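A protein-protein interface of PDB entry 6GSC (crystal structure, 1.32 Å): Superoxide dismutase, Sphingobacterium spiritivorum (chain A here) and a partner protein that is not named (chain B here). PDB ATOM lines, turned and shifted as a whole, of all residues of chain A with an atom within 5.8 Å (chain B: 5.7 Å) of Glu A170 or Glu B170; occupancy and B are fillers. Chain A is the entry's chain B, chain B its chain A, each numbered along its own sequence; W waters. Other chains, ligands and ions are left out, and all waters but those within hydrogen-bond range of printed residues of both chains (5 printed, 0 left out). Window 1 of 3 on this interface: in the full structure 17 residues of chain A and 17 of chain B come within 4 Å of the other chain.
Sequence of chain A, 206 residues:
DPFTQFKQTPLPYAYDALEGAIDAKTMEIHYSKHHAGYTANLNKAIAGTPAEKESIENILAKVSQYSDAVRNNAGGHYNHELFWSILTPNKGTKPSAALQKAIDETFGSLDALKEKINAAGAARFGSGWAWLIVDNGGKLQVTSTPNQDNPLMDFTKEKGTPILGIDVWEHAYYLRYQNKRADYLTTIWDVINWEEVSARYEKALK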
ATOM      1  N   HIS A  34      -6.454  14.992   1.458  1.00  0.00           N
ATOM      2  CA  HIS A  34      -6.753  14.191   0.289  1.00  0.00           C
ATOM      3  C   HIS A  34      -6.574  14.991  -0.979  1.00  0.00           C
ATOM      4  O   HIS A  34      -5.773  14.633  -1.846  1.00  0.00           O
ATOM      5  CB  HIS A  34      -8.156  13.582   0.347  1.00  0.00           C
ATOM      6  CG  HIS A  34      -8.346  12.611   1.473  1.00  0.00           C
ATOM      7  ND1 HIS A  34      -7.710  11.392   1.507  1.00  0.00           N
ATOM      8  CD2 HIS A  34      -9.070  12.673   2.607  1.00  0.00           C
ATOM      9  CE1 HIS A  34      -8.079  10.731   2.598  1.00  0.00           C
ATOM     10  NE2 HIS A  34      -8.863  11.506   3.308  1.00  0.00           N
ATOM     11  N   SER A 127     -14.728   2.780  -3.993  1.00  0.00           N
ATOM     12  CA  SER A 127     -14.549   4.233  -4.011  1.00  0.00           C
ATOM     13  C   SER A 127     -15.031   4.765  -5.326  1.00  0.00           C
ATOM     14  O   SER A 127     -14.855   4.119  -6.359  1.00  0.00           O
ATOM     15  CB  SER A 127     -13.071   4.519  -3.882  1.00  0.00           C
ATOM     16  OG  SER A 127     -12.582   4.023  -2.634  1.00  0.00           O
ATOM     17  N   ASP A 167     -18.769  13.057  -4.293  1.00  0.00           N
ATOM     18  CA  ASP A 167     -17.730  12.117  -3.889  1.00  0.00           C
ATOM     19  C   ASP A 167     -18.335  11.083  -2.990  1.00  0.00           C
ATOM     20  O   ASP A 167     -18.941  11.413  -1.963  1.00  0.00           O
ATOM     21  CB  ASP A 167     -16.693  12.925  -3.146  1.00  0.00           C
ATOM     22  CG  ASP A 167     -15.460  12.180  -2.815  1.00  0.00           C
ATOM     23  OD1 ASP A 167     -15.354  10.936  -3.059  1.00  0.00           O
ATOM     24  OD2 ASP A 167     -14.469  12.844  -2.355  1.00  0.00           O
ATOM     25  N   VAL A 168     -18.227   9.802  -3.383  1.00  0.00           N
ATOM     26  CA  VAL A 168     -18.660   8.727  -2.521  1.00  0.00           C
ATOM     27  C   VAL A 168     -17.529   7.848  -2.076  1.00  0.00           C
ATOM     28  O   VAL A 168     -17.761   6.692  -1.606  1.00  0.00           O
ATOM     29  CB  VAL A 168     -19.839   7.917  -3.092  1.00  0.00           C
ATOM     30  CG1 VAL A 168     -21.084   8.767  -3.249  1.00  0.00           C
ATOM     31  CG2 VAL A 168     -19.517   7.199  -4.415  1.00  0.00           C
ATOM     32  N   TRP A 169     -16.306   8.325  -2.150  1.00  0.00           N
ATOM     33  CA  TRP A 169     -15.262   7.732  -1.345  1.00  0.00           C
ATOM     34  C   TRP A 169     -15.672   7.781   0.125  1.00  0.00           C
ATOM     35  O   TRP A 169     -16.238   8.779   0.574  1.00  0.00           O
ATOM     36  CB  TRP A 169     -13.937   8.474  -1.481  1.00  0.00           C
ATOM     37  CG  TRP A 169     -13.233   8.209  -2.776  1.00  0.00           C
ATOM     38  CD1 TRP A 169     -13.671   8.467  -4.043  1.00  0.00           C
ATOM     39  CD2 TRP A 169     -11.880   7.740  -2.921  1.00  0.00           C
ATOM     40  NE1 TRP A 169     -12.716   8.159  -4.938  1.00  0.00           N
ATOM     41  CE2 TRP A 169     -11.609   7.687  -4.302  1.00  0.00           C
ATOM     42  CE3 TRP A 169     -10.881   7.324  -2.023  1.00  0.00           C
ATOM     43  CZ2 TRP A 169     -10.385   7.248  -4.796  1.00  0.00           C
ATOM     44  CZ3 TRP A 169      -9.687   6.933  -2.499  1.00  0.00           C
ATOM     45  CH2 TRP A 169      -9.445   6.869  -3.899  1.00  0.00           C
ATOM     46  N   GLU A 170     -15.344   6.765   0.914  1.00  0.00           N
ATOM     47  CA  GLU A 170     -15.688   6.754   2.335  1.00  0.00           C
ATOM     48  C   GLU A 170     -15.095   7.937   3.039  1.00  0.00           C
ATOM     49  O   GLU A 170     -15.725   8.424   3.973  1.00  0.00           O
ATOM     50  CB  GLU A 170     -15.369   5.409   2.959  1.00  0.00           C
ATOM     51  CG  GLU A 170     -16.329   4.304   2.498  1.00  0.00           C
ATOM     52  CD  GLU A 170     -15.953   2.861   2.884  1.00  0.00           C
ATOM     53  OE1 GLU A 170     -14.764   2.548   2.931  1.00  0.00           O
ATOM     54  OE2 GLU A 170     -16.937   2.101   3.087  1.00  0.00           O
ATOM     55  N   HIS A 171     -13.937   8.430   2.622  1.00  0.00           N
ATOM     56  CA  HIS A 171     -13.407   9.606   3.321  1.00  0.00           C
ATOM     57  C   HIS A 171     -14.317  10.778   3.275  1.00  0.00           C
ATOM     58  O   HIS A 171     -14.229  11.665   4.128  1.00  0.00           O
ATOM     59  CB  HIS A 171     -11.996   9.954   2.903  1.00  0.00           C
ATOM     60  CG  HIS A 171     -11.832  10.381   1.487  1.00  0.00           C
ATOM     61  ND1 HIS A 171     -10.949   9.766   0.654  1.00  0.00           N
ATOM     62  CD2 HIS A 171     -12.351  11.413   0.776  1.00  0.00           C
ATOM     63  CE1 HIS A 171     -10.956  10.352  -0.534  1.00  0.00           C
ATOM     64  NE2 HIS A 171     -11.780  11.383  -0.481  1.00  0.00           N
ATOM     65  N   ALA A 172     -15.202  10.866   2.301  1.00  0.00           N
ATOM     66  CA  ALA A 172     -16.095  11.978   2.134  1.00  0.00           C
ATOM     67  C   ALA A 172     -17.234  11.975   3.150  1.00  0.00           C
ATOM     68  O   ALA A 172     -17.850  13.010   3.359  1.00  0.00           O
ATOM     69  CB  ALA A 172     -16.659  11.991   0.730  1.00  0.00           C
ATOM     70  N   TYR A 173     -17.522  10.846   3.775  1.00  0.00           N
ATOM     71  CA  TYR A 173     -18.680  10.757   4.631  1.00  0.00           C
ATOM     72  C   TYR A 173     -18.505   9.927   5.870  1.00  0.00           C
ATOM     73  O   TYR A 173     -19.439   9.884   6.687  1.00  0.00           O
ATOM     74  CB  TYR A 173     -19.876  10.245   3.839  1.00  0.00           C
ATOM     75  CG  TYR A 173     -19.753   8.836   3.261  1.00  0.00           C
ATOM     76  CD1 TYR A 173     -20.051   7.712   4.020  1.00  0.00           C
ATOM     77  CD2 TYR A 173     -19.374   8.642   1.938  1.00  0.00           C
ATOM     78  CE1 TYR A 173     -19.971   6.423   3.485  1.00  0.00           C
ATOM     79  CE2 TYR A 173     -19.334   7.364   1.386  1.00  0.00           C
ATOM     80  CZ  TYR A 173     -19.610   6.270   2.180  1.00  0.00           C
ATOM     81  OH  TYR A 173     -19.542   4.998   1.590  1.00  0.00           O
ATOM     82  N   TYR A 174     -17.384   9.256   6.083  1.00  0.00           N
ATOM     83  CA  TYR A 174     -17.361   8.257   7.110  1.00  0.00           C
ATOM     84  C   TYR A 174     -17.390   8.857   8.516  1.00  0.00           C
ATOM     85  O   TYR A 174     -17.948   8.251   9.414  1.00  0.00           O
ATOM     86  CB  TYR A 174     -16.166   7.289   6.938  1.00  0.00           C
ATOM     87  CG  TYR A 174     -16.518   5.888   7.350  1.00  0.00           C
ATOM     88  CD1 TYR A 174     -16.222   5.419   8.595  1.00  0.00           C
ATOM     89  CD2 TYR A 174     -17.319   5.111   6.539  1.00  0.00           C
ATOM     90  CE1 TYR A 174     -16.592   4.140   9.034  1.00  0.00           C
ATOM     91  CE2 TYR A 174     -17.698   3.856   6.962  1.00  0.00           C
ATOM     92  CZ  TYR A 174     -17.381   3.401   8.199  1.00  0.00           C
ATOM     93  OH  TYR A 174     -17.837   2.143   8.554  1.00  0.00           O
ATOM     94  N   LEU A 175     -16.734  10.009   8.745  1.00  0.00           N
ATOM     95  CA  LEU A 175     -16.676  10.554  10.115  1.00  0.00           C
ATOM     96  C   LEU A 175     -18.071  10.876  10.618  1.00  0.00           C
ATOM     97  O   LEU A 175     -18.364  10.626  11.782  1.00  0.00           O
ATOM     98  CB  LEU A 175     -15.778  11.785  10.207  1.00  0.00           C
ATOM     99  CG  LEU A 175     -14.296  11.510   9.980  1.00  0.00           C
ATOM    100  CD1 LEU A 175     -13.555  12.826  10.189  1.00  0.00           C
ATOM    101  CD2 LEU A 175     -13.755  10.444  10.888  1.00  0.00           C
ATOM    102  N   ARG A 181     -23.991   5.703   3.666  1.00  0.00           N
ATOM    103  CA  ARG A 181     -23.760   6.502   2.482  1.00  0.00           C
ATOM    104  C   ARG A 181     -25.055   7.072   1.987  1.00  0.00           C
ATOM    105  O   ARG A 181     -25.075   8.167   1.457  1.00  0.00           O
ATOM    106  CB  ARG A 181     -23.136   5.653   1.383  1.00  0.00           C
ATOM    107  CG  ARG A 181     -22.746   6.459   0.161  1.00  0.00           C
ATOM    108  CD  ARG A 181     -22.366   5.580  -1.021  1.00  0.00           C
ATOM    109  NE  ARG A 181     -21.090   4.923  -0.842  1.00  0.00           N
ATOM    110  CZ  ARG A 181     -20.502   4.190  -1.800  1.00  0.00           C
ATOM    111  NH1 ARG A 181     -21.045   4.060  -3.002  1.00  0.00           N
ATOM    112  NH2 ARG A 181     -19.320   3.619  -1.550  1.00  0.00           N
ATOM    113  N   HIS B  34     -20.872  -3.652   7.658  1.00  0.00           N
ATOM    114  CA  HIS B  34     -20.243  -3.939   6.357  1.00  0.00           C
ATOM    115  C   HIS B  34     -20.191  -5.453   6.110  1.00  0.00           C
ATOM    116  O   HIS B  34     -20.686  -5.933   5.085  1.00  0.00           O
ATOM    117  CB  HIS B  34     -18.852  -3.330   6.258  1.00  0.00           C
ATOM    118  CG  HIS B  34     -18.855  -1.837   6.310  1.00  0.00           C
ATOM    119  ND1 HIS B  34     -19.322  -1.072   5.278  1.00  0.00           N
ATOM    120  CD2 HIS B  34     -18.406  -0.958   7.243  1.00  0.00           C
ATOM    121  CE1 HIS B  34     -19.195   0.214   5.575  1.00  0.00           C
ATOM    122  NE2 HIS B  34     -18.638   0.306   6.757  1.00  0.00           N
ATOM    123  N   SER B 127     -10.314   1.553  -2.776  1.00  0.00           N
ATOM    124  CA  SER B 127     -10.618   0.537  -1.794  1.00  0.00           C
ATOM    125  C   SER B 127      -9.926  -0.771  -2.149  1.00  0.00           C
ATOM    126  O   SER B 127      -9.799  -1.135  -3.330  1.00  0.00           O
ATOM    127  CB  SER B 127     -12.101   0.265  -1.793  1.00  0.00           C
ATOM    128  OG  SER B 127     -12.844   1.457  -1.570  1.00  0.00           O
ATOM    129  N   VAL B 168      -7.820  -2.321   3.494  1.00  0.00           N
ATOM    130  CA  VAL B 168      -7.472  -0.903   3.363  1.00  0.00           C
ATOM    131  C   VAL B 168      -8.591  -0.134   2.733  1.00  0.00           C
ATOM    132  O   VAL B 168      -8.365   0.990   2.282  1.00  0.00           O
ATOM    133  CB  VAL B 168      -6.129  -0.701   2.653  1.00  0.00           C
ATOM    134  CG1 VAL B 168      -5.014  -1.261   3.506  1.00  0.00           C
ATOM    135  CG2 VAL B 168      -6.082  -1.270   1.271  1.00  0.00           C
ATOM    136  N   TRP B 169      -9.816  -0.648   2.741  1.00  0.00           N
ATOM    137  CA  TRP B 169     -10.968   0.238   2.569  1.00  0.00           C
ATOM    138  C   TRP B 169     -10.895   1.313   3.678  1.00  0.00           C
ATOM    139  O   TRP B 169     -10.567   1.028   4.829  1.00  0.00           O
ATOM    140  CB  TRP B 169     -12.299  -0.505   2.715  1.00  0.00           C
ATOM    141  CG  TRP B 169     -12.633  -1.415   1.558  1.00  0.00           C
ATOM    142  CD1 TRP B 169     -11.921  -2.432   1.072  1.00  0.00           C
ATOM    143  CD2 TRP B 169     -13.820  -1.329   0.809  1.00  0.00           C
ATOM    144  NE1 TRP B 169     -12.596  -2.981   0.036  1.00  0.00           N
ATOM    145  CE2 TRP B 169     -13.779  -2.360  -0.149  1.00  0.00           C
ATOM    146  CE3 TRP B 169     -14.941  -0.510   0.847  1.00  0.00           C
ATOM    147  CZ2 TRP B 169     -14.816  -2.571  -1.058  1.00  0.00           C
ATOM    148  CZ3 TRP B 169     -15.992  -0.715  -0.061  1.00  0.00           C
ATOM    149  CH2 TRP B 169     -15.916  -1.748  -0.991  1.00  0.00           C
ATOM    150  N   GLU B 170     -11.317   2.519   3.341  1.00  0.00           N
ATOM    151  CA  GLU B 170     -11.313   3.583   4.328  1.00  0.00           C
ATOM    152  C   GLU B 170     -12.181   3.264   5.510  1.00  0.00           C
ATOM    153  O   GLU B 170     -11.863   3.696   6.630  1.00  0.00           O
ATOM    154  CB  GLU B 170     -11.647   4.902   3.632  1.00  0.00           C
ATOM    155  CG  GLU B 170     -10.503   5.455   2.823  1.00  0.00           C
ATOM    156  CD  GLU B 170     -10.801   6.706   1.988  1.00  0.00           C
ATOM    157  OE1 GLU B 170     -11.919   6.831   1.486  1.00  0.00           O
ATOM    158  OE2 GLU B 170      -9.795   7.439   1.769  1.00  0.00           O
ATOM    159  N   HIS B 171     -13.260   2.535   5.347  1.00  0.00           N
ATOM    160  CA  HIS B 171     -14.064   2.189   6.538  1.00  0.00           C
ATOM    161  C   HIS B 171     -13.267   1.404   7.572  1.00  0.00           C
ATOM    162  O   HIS B 171     -13.676   1.356   8.733  1.00  0.00           O
ATOM    163  CB  HIS B 171     -15.367   1.463   6.198  1.00  0.00           C
ATOM    164  CG  HIS B 171     -15.188   0.112   5.526  1.00  0.00           C
ATOM    165  ND1 HIS B 171     -15.760  -0.170   4.304  1.00  0.00           N
ATOM    166  CD2 HIS B 171     -14.641  -1.060   5.943  1.00  0.00           C
ATOM    167  CE1 HIS B 171     -15.541  -1.448   3.989  1.00  0.00           C
ATOM    168  NE2 HIS B 171     -14.867  -2.011   4.956  1.00  0.00           N
ATOM    169  N   ALA B 172     -12.183   0.761   7.183  1.00  0.00           N
ATOM    170  CA  ALA B 172     -11.387  -0.014   8.121  1.00  0.00           C
ATOM    171  C   ALA B 172     -10.589   0.869   9.053  1.00  0.00           C
ATOM    172  O   ALA B 172     -10.135   0.366  10.074  1.00  0.00           O
ATOM    173  CB  ALA B 172     -10.490  -0.997   7.351  1.00  0.00           C
ATOM    174  N   TYR B 173     -10.313   2.096   8.665  1.00  0.00           N
ATOM    175  CA  TYR B 173      -9.378   2.884   9.433  1.00  0.00           C
ATOM    176  C   TYR B 173      -9.744   4.353   9.593  1.00  0.00           C
ATOM    177  O   TYR B 173      -9.024   5.099  10.300  1.00  0.00           O
ATOM    178  CB  TYR B 173      -7.968   2.840   8.834  1.00  0.00           C
ATOM    179  CG  TYR B 173      -7.818   3.342   7.418  1.00  0.00           C
ATOM    180  CD1 TYR B 173      -7.588   4.665   7.121  1.00  0.00           C
ATOM    181  CD2 TYR B 173      -7.844   2.444   6.345  1.00  0.00           C
ATOM    182  CE1 TYR B 173      -7.432   5.105   5.839  1.00  0.00           C
ATOM    183  CE2 TYR B 173      -7.674   2.870   5.064  1.00  0.00           C
ATOM    184  CZ  TYR B 173      -7.433   4.199   4.812  1.00  0.00           C
ATOM    185  OH  TYR B 173      -7.241   4.643   3.517  1.00  0.00           O
ATOM    186  N   TYR B 174     -10.802   4.828   8.988  1.00  0.00           N
ATOM    187  CA  TYR B 174     -10.994   6.276   8.918  1.00  0.00           C
ATOM    188  C   TYR B 174     -11.358   6.847  10.264  1.00  0.00           C
ATOM    189  O   TYR B 174     -10.950   8.003  10.556  1.00  0.00           O
ATOM    190  CB  TYR B 174     -12.045   6.657   7.859  1.00  0.00           C
ATOM    191  CG  TYR B 174     -11.636   7.951   7.197  1.00  0.00           C
ATOM    192  CD1 TYR B 174     -12.187   9.182   7.569  1.00  0.00           C
ATOM    193  CD2 TYR B 174     -10.619   7.980   6.255  1.00  0.00           C
ATOM    194  CE1 TYR B 174     -11.745  10.363   6.994  1.00  0.00           C
ATOM    195  CE2 TYR B 174     -10.164   9.140   5.681  1.00  0.00           C
ATOM    196  CZ  TYR B 174     -10.711  10.347   6.086  1.00  0.00           C
ATOM    197  OH  TYR B 174     -10.295  11.530   5.506  1.00  0.00           O
ATOM    198  N   LEU B 175     -12.172   6.190  11.071  1.00  0.00           N
ATOM    199  CA  LEU B 175     -12.549   6.801  12.338  1.00  0.00           C
ATOM    200  C   LEU B 175     -11.360   7.056  13.219  1.00  0.00           C
ATOM    201  O   LEU B 175     -11.367   8.104  13.933  1.00  0.00           O
ATOM    202  CB  LEU B 175     -13.577   5.957  13.065  1.00  0.00           C
ATOM    203  CG  LEU B 175     -14.920   5.829  12.371  1.00  0.00           C
ATOM    204  CD1 LEU B 175     -15.892   5.031  13.235  1.00  0.00           C
ATOM    205  CD2 LEU B 175     -15.546   7.168  12.001  1.00  0.00           C
ATOM    206  N   ARG B 181      -3.529   6.248   6.375  1.00  0.00           N
ATOM    207  CA  ARG B 181      -3.496   4.798   6.128  1.00  0.00           C
ATOM    208  C   ARG B 181      -2.171   4.166   6.502  1.00  0.00           C
ATOM    209  O   ARG B 181      -2.148   3.057   7.030  1.00  0.00           O
ATOM    210  CB  ARG B 181      -3.825   4.508   4.674  1.00  0.00           C
ATOM    211  CG  ARG B 181      -3.957   3.023   4.366  1.00  0.00           C
ATOM    212  CD  ARG B 181      -3.954   2.665   2.897  1.00  0.00           C
ATOM    213  NE  ARG B 181      -5.162   3.089   2.261  1.00  0.00           N
ATOM    214  CZ  ARG B 181      -5.435   2.843   0.987  1.00  0.00           C
ATOM    215  NH1 ARG B 181      -4.619   2.106   0.263  1.00  0.00           N
ATOM    216  NH2 ARG B 181      -6.544   3.319   0.450  1.00  0.00           N
HETATM  217  O   HOH W   1     -12.949   2.610   0.915  1.00  0.00           O
HETATM  218  O   HOH W   2     -16.170   0.266   9.745  1.00  0.00           O
HETATM  219  O   HOH W   3     -11.998  13.469   4.542  1.00  0.00           O
HETATM  220  O   HOH W   4     -12.314   1.435  -4.988  1.00  0.00           O
HETATM  221  O   HOH W   5     -13.226   5.035  -0.157  1.00  0.00           O
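The side-chain carboxylate of Asp A167 sits at hydrogen-bond distance from the backbone NH of Trp A169, 2.9 Å away.
CE1 of His A34 touches OE2 of Glu B170 (3.8 Å). Glu B170 touches Trp A169. CE1 of His B34 touches OE2 of Glu A170 (3.9 Å). Trp B169 touches Glu A170. Tyr B174 touches His A171 (CE2 to CB, 3.4 Å). His B171 touches Tyr A174. O of Tyr A174 touches CD2 of Leu B175, 3.7 Å away. CD2 of Leu A175 touches O of Tyr B174, at 3.7 Å. Leu A175 touches Leu B175 (CD2 to CD2, 3.9 Å).
Water W1 lies within hydrogen-bond range of the side-chain carboxylate (OE1) of Glu A170 (2.7 Å), the side-chain hydroxyl (OG) of Ser B127 (2.7 Å) and the backbone NH (N) of Glu B170 (2.9 Å). Water W5 lies within hydrogen-bond range of OG of Ser A127 (2.8 Å), OE1 of Glu B170 (2.8 Å) and N of Glu A170 (2.9 Å). Water W3 lies within hydrogen-bond range of OH of Tyr B174 and O of His A171. Water W2 bridges OH of Tyr A174 (2.8 Å) and O of His B171 (2.9 Å). Water W4 bridges the backbone NH of Ser A127 (2.9 Å) and the backbone NH of Ser B127 (3.0 Å).
Of the printed residues of chain B, His A34 touches Glu B170 (3.8 Å) and Tyr B174 (2.6 Å). Printed residues of chain B within 4 Å of Trp A169: Glu B170. Glu A170 touches just these residues of chain B: His B34, Trp B169, Glu B170 and His B171. Of the printed residues of chain B, His A171 touches Glu B170 and Tyr B174. Of the printed residues of chain B, Tyr A174 touches His B34 (2.7 Å), His B171 (3.4 Å) and Leu B175 (3.7 Å). Arg A181 touches none of the printed residues of chain B. Printed residues of chain A within 4 Å of Trp B169: Glu A170. Of chain A, only His A34 (3.8 Å), Trp A169 (3.7 Å), Glu A170 (3.5 Å) and His A171 (2.8 Å) come within 4 Å of Glu B170. The nearest residue of chain B that does not touch Glu A170 is Ser B127 (5.0 Å). The nearest printed residue of chain A that does not touch His B34 is Tyr A173 (6.2 Å).
The backbone NH (N) of His A171 lies within hydrogen-bond range of the side-chain carboxylate (OE1) of Glu B170, 2.8 Å away. The side-chain carboxylate (OE1) of Glu A170 sits at hydrogen-bond distance from the backbone NH (N) of Glu B170 (3.5 Å). The side-chain carboxylate of Glu A170 sits at hydrogen-bond distance from a ring nitrogen (ND1) of His B171 (2.8 Å). NE2 of His B34 lies within hydrogen-bond range of OH of Tyr A174. The side-chain hydroxyl (OG) of Ser B127 is in hydrogen-bond range of the side-chain hydroxyl (OG) of Ser A127 (2.8 Å). A ring nitrogen (NE2) of His A34 lies within hydrogen-bond range of the side-chain hydroxyl of Tyr B174, at 2.6 Å.
Of the 11 printed residues of chain B, 7 touch a printed residue of chain A. Hydrophobic or aromatic side chains of chain B within 4 Å of the printed part of chain A: His B34, Trp B169, His B171, Tyr B174 and Leu B175. Printed residues of chain A that touch a printed residue of chain B: His A34, Ser A127, Trp A169, Glu A170, His A171, Tyr A174 and Leu A175. Among the printed residues, no Asp or Glu carboxylate lies within 4 Å of a Lys or Arg side-chain nitrogen of the other chain.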
